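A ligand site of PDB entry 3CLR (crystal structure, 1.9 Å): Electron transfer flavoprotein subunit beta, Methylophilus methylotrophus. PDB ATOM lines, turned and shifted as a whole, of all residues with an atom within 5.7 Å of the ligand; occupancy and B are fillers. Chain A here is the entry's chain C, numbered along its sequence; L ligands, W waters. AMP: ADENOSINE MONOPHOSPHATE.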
ATOM      1  N   ALA A   6     -21.673  12.250  19.379  1.00  0.00           N
ATOM      2  CA  ALA A   6     -20.499  12.299  18.531  1.00  0.00           C
ATOM      3  C   ALA A   6     -20.931  12.808  17.164  1.00  0.00           C
ATOM      4  O   ALA A   6     -21.877  12.274  16.576  1.00  0.00           O
ATOM      5  CB  ALA A   6     -19.863  10.885  18.419  1.00  0.00           C
ATOM      6  N   VAL A   7     -20.252  13.858  16.669  1.00  0.00           N
ATOM      7  CA  VAL A   7     -20.573  14.448  15.375  1.00  0.00           C
ATOM      8  C   VAL A   7     -19.350  14.580  14.490  1.00  0.00           C
ATOM      9  O   VAL A   7     -18.229  14.794  14.961  1.00  0.00           O
ATOM     10  CB  VAL A   7     -21.329  15.808  15.508  1.00  0.00           C
ATOM     11  CG1 VAL A   7     -22.551  15.656  16.406  1.00  0.00           C
ATOM     12  CG2 VAL A   7     -20.432  16.928  16.060  1.00  0.00           C
ATOM     13  N   LYS A   8     -19.584  14.440  13.194  1.00  0.00           N
ATOM     14  CA  LYS A   8     -18.558  14.579  12.165  1.00  0.00           C
ATOM     15  C   LYS A   8     -18.946  15.697  11.176  1.00  0.00           C
ATOM     16  O   LYS A   8     -20.079  15.801  10.702  1.00  0.00           O
ATOM     17  CB  LYS A   8     -18.383  13.275  11.390  1.00  0.00           C
ATOM     18  CG  LYS A   8     -17.219  13.304  10.437  1.00  0.00           C
ATOM     19  CD  LYS A   8     -17.108  12.059   9.581  1.00  0.00           C
ATOM     20  CE  LYS A   8     -15.936  12.194   8.626  1.00  0.00           C
ATOM     21  NZ  LYS A   8     -15.774  10.953   7.717  1.00  0.00           N
ATOM     22  N   ASN A  36     -22.377  16.325   9.160  1.00  0.00           N
ATOM     23  CA  ASN A  36     -22.933  15.069   8.643  1.00  0.00           C
ATOM     24  C   ASN A  36     -24.459  15.043   8.831  1.00  0.00           C
ATOM     25  O   ASN A  36     -24.962  15.355   9.905  1.00  0.00           O
ATOM     26  CB  ASN A  36     -22.286  13.870   9.352  1.00  0.00           C
ATOM     27  CG  ASN A  36     -22.756  12.540   8.793  1.00  0.00           C
ATOM     28  OD1 ASN A  36     -22.979  12.404   7.569  1.00  0.00           O
ATOM     29  ND2 ASN A  36     -22.964  11.557   9.688  1.00  0.00           N
ATOM     30  N   TRP A  38     -26.689  12.698   9.220  1.00  0.00           N
ATOM     31  CA  TRP A  38     -27.131  11.826  10.293  1.00  0.00           C
ATOM     32  C   TRP A  38     -26.992  12.510  11.666  1.00  0.00           C
ATOM     33  O   TRP A  38     -27.813  12.269  12.557  1.00  0.00           O
ATOM     34  CB  TRP A  38     -26.330  10.500  10.259  1.00  0.00           C
ATOM     35  CG  TRP A  38     -26.885   9.531   9.287  1.00  0.00           C
ATOM     36  CD1 TRP A  38     -27.786   8.547   9.544  1.00  0.00           C
ATOM     37  CD2 TRP A  38     -26.609   9.465   7.884  1.00  0.00           C
ATOM     38  NE1 TRP A  38     -28.075   7.848   8.377  1.00  0.00           N
ATOM     39  CE2 TRP A  38     -27.363   8.394   7.345  1.00  0.00           C
ATOM     40  CE3 TRP A  38     -25.734  10.189   7.025  1.00  0.00           C
ATOM     41  CZ2 TRP A  38     -27.351   8.065   6.005  1.00  0.00           C
ATOM     42  CZ3 TRP A  38     -25.719   9.854   5.697  1.00  0.00           C
ATOM     43  CH2 TRP A  38     -26.509   8.799   5.195  1.00  0.00           C
ATOM     44  N   ASP A  39     -26.013  13.402  11.824  1.00  0.00           N
ATOM     45  CA  ASP A  39     -25.820  14.107  13.089  1.00  0.00           C
ATOM     46  C   ASP A  39     -26.890  15.167  13.386  1.00  0.00           C
ATOM     47  O   ASP A  39     -27.179  15.440  14.569  1.00  0.00           O
ATOM     48  CB  ASP A  39     -24.412  14.702  13.177  1.00  0.00           C
ATOM     49  CG  ASP A  39     -23.351  13.635  13.134  1.00  0.00           C
ATOM     50  OD1 ASP A  39     -23.596  12.527  13.682  1.00  0.00           O
ATOM     51  OD2 ASP A  39     -22.279  13.883  12.548  1.00  0.00           O
ATOM     52  N   VAL A  62     -19.408  16.241  20.456  1.00  0.00           N
ATOM     53  CA  VAL A  62     -17.964  15.987  20.456  1.00  0.00           C
ATOM     54  C   VAL A  62     -17.539  15.602  19.068  1.00  0.00           C
ATOM     55  O   VAL A  62     -18.184  14.753  18.459  1.00  0.00           O
ATOM     56  CB  VAL A  62     -17.544  14.847  21.429  1.00  0.00           C
ATOM     57  CG1 VAL A  62     -16.021  14.613  21.412  1.00  0.00           C
ATOM     58  CG2 VAL A  62     -18.006  15.154  22.815  1.00  0.00           C
ATOM     59  N   SER A  63     -16.446  16.182  18.585  1.00  0.00           N
ATOM     60  CA  SER A  63     -15.930  15.849  17.250  1.00  0.00           C
ATOM     61  C   SER A  63     -14.437  15.745  17.288  1.00  0.00           C
ATOM     62  O   SER A  63     -13.772  16.539  17.921  1.00  0.00           O
ATOM     63  CB  SER A  63     -16.343  16.892  16.186  1.00  0.00           C
ATOM     64  OG  SER A  63     -16.128  16.412  14.843  1.00  0.00           O
ATOM     65  N   VAL A  64     -13.923  14.733  16.598  1.00  0.00           N
ATOM     66  CA  VAL A  64     -12.508  14.600  16.352  1.00  0.00           C
ATOM     67  C   VAL A  64     -12.180  15.157  14.948  1.00  0.00           C
ATOM     68  O   VAL A  64     -12.584  14.602  13.927  1.00  0.00           O
ATOM     69  CB  VAL A  64     -12.110  13.150  16.447  1.00  0.00           C
ATOM     70  CG1 VAL A  64     -10.609  12.999  16.268  1.00  0.00           C
ATOM     71  CG2 VAL A  64     -12.557  12.535  17.806  1.00  0.00           C
ATOM     72  N   GLY A  65     -11.456  16.260  14.898  1.00  0.00           N
ATOM     73  CA  GLY A  65     -11.080  16.795  13.621  1.00  0.00           C
ATOM     74  C   GLY A  65     -10.353  18.100  13.763  1.00  0.00           C
ATOM     75  O   GLY A  65     -10.300  18.662  14.853  1.00  0.00           O
ATOM     76  N   ALA A  97     -12.142   4.747  11.230  1.00  0.00           N
ATOM     77  CA  ALA A  97     -13.333   4.708  12.125  1.00  0.00           C
ATOM     78  C   ALA A  97     -13.014   4.093  13.486  1.00  0.00           C
ATOM     79  O   ALA A  97     -13.577   4.494  14.502  1.00  0.00           O
ATOM     80  CB  ALA A  97     -14.434   3.939  11.495  1.00  0.00           C
ATOM     81  N   VAL A 100     -10.776   6.558  15.403  1.00  0.00           N
ATOM     82  CA  VAL A 100     -11.641   7.641  15.890  1.00  0.00           C
ATOM     83  C   VAL A 100     -12.513   7.146  17.051  1.00  0.00           C
ATOM     84  O   VAL A 100     -12.705   7.862  18.055  1.00  0.00           O
ATOM     85  CB  VAL A 100     -12.468   8.329  14.751  1.00  0.00           C
ATOM     86  CG1 VAL A 100     -13.549   9.247  15.297  1.00  0.00           C
ATOM     87  CG2 VAL A 100     -11.515   9.150  13.858  1.00  0.00           C
ATOM     88  N   LEU A 104     -12.622   8.980  20.629  1.00  0.00           N
ATOM     89  CA  LEU A 104     -13.899   9.391  21.207  1.00  0.00           C
ATOM     90  C   LEU A 104     -14.110   8.810  22.581  1.00  0.00           C
ATOM     91  O   LEU A 104     -14.513   9.509  23.503  1.00  0.00           O
ATOM     92  CB  LEU A 104     -15.051   9.018  20.282  1.00  0.00           C
ATOM     93  CG  LEU A 104     -15.193   9.914  19.048  1.00  0.00           C
ATOM     94  CD1 LEU A 104     -16.184   9.311  18.095  1.00  0.00           C
ATOM     95  CD2 LEU A 104     -15.649  11.299  19.432  1.00  0.00           C
ATOM     96  N   PHE A 117     -24.957   8.983  21.512  1.00  0.00           N
ATOM     97  CA  PHE A 117     -25.540   8.915  20.182  1.00  0.00           C
ATOM     98  C   PHE A 117     -24.446   9.159  19.125  1.00  0.00           C
ATOM     99  O   PHE A 117     -23.570  10.029  19.255  1.00  0.00           O
ATOM    100  CB  PHE A 117     -26.651   9.940  19.978  1.00  0.00           C
ATOM    101  CG  PHE A 117     -27.858   9.782  20.895  1.00  0.00           C
ATOM    102  CD1 PHE A 117     -28.080   8.661  21.713  1.00  0.00           C
ATOM    103  CD2 PHE A 117     -28.837  10.774  20.871  1.00  0.00           C
ATOM    104  CE1 PHE A 117     -29.214   8.588  22.526  1.00  0.00           C
ATOM    105  CE2 PHE A 117     -29.972  10.706  21.639  1.00  0.00           C
ATOM    106  CZ  PHE A 117     -30.168   9.613  22.468  1.00  0.00           C
ATOM    107  N   ALA A 118     -24.508   8.351  18.078  1.00  0.00           N
ATOM    108  CA  ALA A 118     -23.720   8.524  16.860  1.00  0.00           C
ATOM    109  C   ALA A 118     -24.650   8.404  15.673  1.00  0.00           C
ATOM    110  O   ALA A 118     -25.743   7.817  15.776  1.00  0.00           O
ATOM    111  CB  ALA A 118     -22.637   7.455  16.773  1.00  0.00           C
ATOM    112  N   GLY A 119     -24.197   8.889  14.527  1.00  0.00           N
ATOM    113  CA  GLY A 119     -24.947   8.693  13.300  1.00  0.00           C
ATOM    114  C   GLY A 119     -24.753   7.275  12.776  1.00  0.00           C
ATOM    115  O   GLY A 119     -23.733   6.616  13.069  1.00  0.00           O
ATOM    116  N   VAL A 120     -25.704   6.780  11.993  1.00  0.00           N
ATOM    117  CA  VAL A 120     -25.540   5.434  11.382  1.00  0.00           C
ATOM    118  C   VAL A 120     -24.279   5.377  10.539  1.00  0.00           C
ATOM    119  O   VAL A 120     -23.545   4.366  10.564  1.00  0.00           O
ATOM    120  CB  VAL A 120     -26.783   5.008  10.515  1.00  0.00           C
ATOM    121  CG1 VAL A 120     -26.477   3.902   9.502  1.00  0.00           C
ATOM    122  CG2 VAL A 120     -27.916   4.586  11.406  1.00  0.00           C
ATOM    123  N   GLN A 121     -24.045   6.444   9.764  1.00  0.00           N
ATOM    124  CA  GLN A 121     -22.874   6.520   8.890  1.00  0.00           C
ATOM    125  C   GLN A 121     -22.590   7.970   8.521  1.00  0.00           C
ATOM    126  O   GLN A 121     -23.390   8.880   8.838  1.00  0.00           O
ATOM    127  CB  GLN A 121     -23.066   5.667   7.646  1.00  0.00           C
ATOM    128  CG  GLN A 121     -24.109   6.204   6.676  1.00  0.00           C
ATOM    129  CD  GLN A 121     -24.261   5.343   5.431  1.00  0.00           C
ATOM    130  OE1 GLN A 121     -24.349   5.878   4.324  1.00  0.00           O
ATOM    131  NE2 GLN A 121     -24.232   4.036   5.612  1.00  0.00           N
ATOM    132  N   SER A 122     -21.409   8.196   7.923  1.00  0.00           N
ATOM    133  CA  SER A 122     -21.019   9.508   7.379  1.00  0.00           C
ATOM    134  C   SER A 122     -21.354   9.571   5.897  1.00  0.00           C
ATOM    135  O   SER A 122     -21.217   8.567   5.185  1.00  0.00           O
ATOM    136  CB  SER A 122     -19.520   9.802   7.565  1.00  0.00           C
ATOM    137  OG  SER A 122     -18.704   8.725   7.175  1.00  0.00           O
ATOM    138  N   GLN A 125     -17.536   9.079   3.752  1.00  0.00           N
ATOM    139  CA  GLN A 125     -16.937   7.746   3.695  1.00  0.00           C
ATOM    140  C   GLN A 125     -17.915   6.577   3.924  1.00  0.00           C
ATOM    141  O   GLN A 125     -17.636   5.445   3.470  1.00  0.00           O
ATOM    142  CB  GLN A 125     -15.709   7.671   4.595  1.00  0.00           C
ATOM    143  CG  GLN A 125     -14.570   8.756   4.284  1.00  0.00           C
ATOM    144  CD  GLN A 125     -14.547   9.456   2.853  1.00  0.00           C
ATOM    145  OE1 GLN A 125     -14.789   8.870   1.826  1.00  0.00           O
ATOM    146  NE2 GLN A 125     -14.158  10.713   2.851  1.00  0.00           N
ATOM    147  N   ALA A 126     -19.039   6.824   4.611  1.00  0.00           N
ATOM    148  CA  ALA A 126     -20.033   5.811   4.834  1.00  0.00           C
ATOM    149  C   ALA A 126     -19.397   4.499   5.287  1.00  0.00           C
ATOM    150  O   ALA A 126     -19.638   3.435   4.703  1.00  0.00           O
ATOM    151  CB  ALA A 126     -20.836   5.607   3.570  1.00  0.00           C
ATOM    152  N   TYR A 127     -18.592   4.599   6.346  1.00  0.00           N
ATOM    153  CA  TYR A 127     -18.001   3.423   6.947  1.00  0.00           C
ATOM    154  C   TYR A 127     -19.066   2.639   7.715  1.00  0.00           C
ATOM    155  O   TYR A 127     -18.931   1.419   7.822  1.00  0.00           O
ATOM    156  CB  TYR A 127     -16.918   3.767   7.963  1.00  0.00           C
ATOM    157  CG  TYR A 127     -15.733   4.512   7.415  1.00  0.00           C
ATOM    158  CD1 TYR A 127     -15.324   5.715   7.974  1.00  0.00           C
ATOM    159  CD2 TYR A 127     -14.980   3.987   6.356  1.00  0.00           C
ATOM    160  CE1 TYR A 127     -14.198   6.401   7.501  1.00  0.00           C
ATOM    161  CE2 TYR A 127     -13.866   4.671   5.844  1.00  0.00           C
ATOM    162  CZ  TYR A 127     -13.478   5.889   6.414  1.00  0.00           C
ATOM    163  OH  TYR A 127     -12.360   6.587   5.891  1.00  0.00           O
ATOM    164  N   ALA A 128     -20.051   3.358   8.265  1.00  0.00           N
ATOM    165  CA  ALA A 128     -21.038   2.824   9.213  1.00  0.00           C
ATOM    166  C   ALA A 128     -20.345   1.957  10.296  1.00  0.00           C
ATOM    167  O   ALA A 128     -20.726   0.782  10.500  1.00  0.00           O
ATOM    168  CB  ALA A 128     -22.095   2.051   8.494  1.00  0.00           C
ATOM    169  N   SER A 129     -19.317   2.542  10.922  1.00  0.00           N
ATOM    170  CA  SER A 129     -18.436   1.834  11.843  1.00  0.00           C
ATOM    171  C   SER A 129     -18.088   2.546  13.129  1.00  0.00           C
ATOM    172  O   SER A 129     -17.797   1.904  14.119  1.00  0.00           O
ATOM    173  CB  SER A 129     -17.091   1.544  11.157  1.00  0.00           C
ATOM    174  OG  SER A 129     -17.213   0.562  10.157  1.00  0.00           O
ATOM    175  N   THR A 130     -18.037   3.868  13.087  1.00  0.00           N
ATOM    176  CA  THR A 130     -17.463   4.640  14.203  1.00  0.00           C
ATOM    177  C   THR A 130     -18.219   4.485  15.513  1.00  0.00           C
ATOM    178  O   THR A 130     -17.623   4.226  16.578  1.00  0.00           O
ATOM    179  CB  THR A 130     -17.311   6.123  13.765  1.00  0.00           C
ATOM    180  OG1 THR A 130     -16.508   6.171  12.585  1.00  0.00           O
ATOM    181  CG2 THR A 130     -16.601   6.941  14.845  1.00  0.00           C
ATOM    182  N   GLY A 131     -19.530   4.664  15.472  1.00  0.00           N
ATOM    183  CA  GLY A 131     -20.292   4.590  16.697  1.00  0.00           C
ATOM    184  C   GLY A 131     -20.205   3.231  17.381  1.00  0.00           C
ATOM    185  O   GLY A 131     -20.075   3.134  18.595  1.00  0.00           O
HETATM  186  P   AMP L   1     -19.079   6.458  10.047  1.00  0.00           P
HETATM  187  O1P AMP L   1     -18.052   7.542  10.105  1.00  0.00           O
HETATM  188  O2P AMP L   1     -18.693   5.210  10.729  1.00  0.00           O
HETATM  189  O3P AMP L   1     -19.540   6.222   8.653  1.00  0.00           O
HETATM  190  O5' AMP L   1     -20.321   7.033  10.913  1.00  0.00           O
HETATM  191  C5' AMP L   1     -20.539   8.412  11.091  1.00  0.00           C
HETATM  192  C4' AMP L   1     -20.936   8.742  12.519  1.00  0.00           C
HETATM  193  O4' AMP L   1     -19.883   8.350  13.418  1.00  0.00           O
HETATM  194  C3' AMP L   1     -21.135  10.233  12.689  1.00  0.00           C
HETATM  195  O3' AMP L   1     -22.504  10.555  12.521  1.00  0.00           O
HETATM  196  C2' AMP L   1     -20.600  10.475  14.075  1.00  0.00           C
HETATM  197  O2' AMP L   1     -21.598  10.199  15.069  1.00  0.00           O
HETATM  198  C1' AMP L   1     -19.495   9.445  14.197  1.00  0.00           C
HETATM  199  N9  AMP L   1     -18.208   9.988  13.723  1.00  0.00           N
HETATM  200  C8  AMP L   1     -17.477   9.611  12.656  1.00  0.00           C
HETATM  201  N7  AMP L   1     -16.340  10.334  12.600  1.00  0.00           N
HETATM  202  C5  AMP L   1     -16.349  11.150  13.646  1.00  0.00           C
HETATM  203  C6  AMP L   1     -15.433  12.167  14.134  1.00  0.00           C
HETATM  204  N6  AMP L   1     -14.303  12.409  13.431  1.00  0.00           N
HETATM  205  N1  AMP L   1     -15.750  12.814  15.280  1.00  0.00           N
HETATM  206  C2  AMP L   1     -16.897  12.514  15.955  1.00  0.00           C
HETATM  207  N3  AMP L   1     -17.799  11.593  15.547  1.00  0.00           N
HETATM  208  C4  AMP L   1     -17.557  10.912  14.409  1.00  0.00           C
HETATM  209  O   HOH W   1     -11.035  12.825  12.256  1.00  0.00           O
HETATM  210  O   HOH W   2     -16.023   8.724   9.260  1.00  0.00           O
HETATM  211  O   HOH W   3     -21.251   5.113  13.048  1.00  0.00           O
HETATM  212  O   HOH W   4     -12.941  11.511  10.852  1.00  0.00           O
HETATM  213  O   HOH W   5     -24.452  11.781  16.210  1.00  0.00           O
HETATM  214  O   HOH W   6     -14.586   8.095  11.832  1.00  0.00           O
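OD2 of Asp 39 sits at hydrogen-bond distance from N of Lys 8 (2.8 Å).
O of Phe 117 sits at hydrogen-bond distance from N of Ala 6 (2.9 Å).
The side-chain hydroxyl of Ser 129 lies within hydrogen-bond range of the backbone carbonyl oxygen of Tyr 127, 3.0 Å away.
The side-chain hydroxyl (OG) of Ser 122 sits at hydrogen-bond distance from the backbone NH (N) of Ala 126, at 3.2 Å.
N of Val 7 sits at hydrogen-bond distance from O of Val 62 (2.9 Å).
The backbone carbonyl oxygen (O) of Val 7 lies within hydrogen-bond range of the side-chain hydroxyl (OG) of Ser 63, 2.7 Å away.
The side-chain amide nitrogen (ND2) of Asn 36 sits at hydrogen-bond distance from the backbone carbonyl oxygen (O) of Gln 121.
The backbone NH (N) of Asn 36 sits at hydrogen-bond distance from the backbone carbonyl oxygen (O) of Lys 8.
Water W2 lies within hydrogen-bond range of an oxygen (O1P) of the ligand (2.5 Å), the side-chain amino group (NZ) of Lys 8 (2.7 Å) and the side-chain hydroxyl (OG) of Ser 122 (3.4 Å).
Water W6 bridges the side-chain hydroxyl of Thr 130 and a nitrogen (N7) of the ligand.
Water W5 lies within hydrogen-bond range of O of Ala 6, OD1 of Asp 39, N of Gly 119 and O2' of the ligand.
Water W1 bridges O of Val 64 and N6 of the ligand.
A nitrogen (N1) of the ligand lies close to the backbone carbonyl oxygen (O) of Val 7 (3.2 Å).
Lys 8 touches the ligand.
Val 62 touches the ligand (O to C2, 3.6 Å).
Ser 63 touches the ligand (CA to N1, 3.6 Å).
Val 100 touches the ligand (CG1 to C6, 3.7 Å).
Leu 104 touches the ligand.
Ala 118 touches the ligand.
Gln 121 touches the ligand.
C of Ala 126 touches O3P of the ligand, at 3.8 Å.
Hydrophobic or aromatic side chains that line the ligand: Ala 6, Val 64, Val 100, Leu 104, Ala 118 and Tyr 127.
An oxygen (O3') of the ligand lies within hydrogen-bond range of the side-chain carboxylate of Asp 39, at 2.5 Å.
The backbone carbonyl oxygen (O) of Ala 6 sits at hydrogen-bond distance from an oxygen (O2') of the ligand (2.6 Å).
N of Ser 129 is in hydrogen-bond range of O2P of the ligand.
An oxygen (O2P) of the ligand is in hydrogen-bond range of the backbone NH (N) of Thr 130, 2.8 Å away.
O2P of the ligand lies within hydrogen-bond range of OG1 of Thr 130 (3.0 Å).
The backbone NH (N) of Ser 122 sits at hydrogen-bond distance from an oxygen (O3P) of the ligand (2.8 Å).
O3P of the ligand sits at hydrogen-bond distance from OG of Ser 122 (3.0 Å).
The backbone NH (N) of Val 64 sits at hydrogen-bond distance from a nitrogen (N1) of the ligand (3.0 Å).
The backbone carbonyl oxygen of Val 64 is in hydrogen-bond range of a nitrogen (N6) of the ligand, at 2.8 Å.
The backbone NH of Ala 128 is in hydrogen-bond range of an oxygen (O3P) of the ligand (2.9 Å).
N of Gly 119 sits at hydrogen-bond distance from O2' of the ligand (3.0 Å).
N of Tyr 127 sits at hydrogen-bond distance from O3P of the ligand, 3.0 Å away.
ND2 of Asn 36 lies within hydrogen-bond range of O3' of the ligand (3.0 Å).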
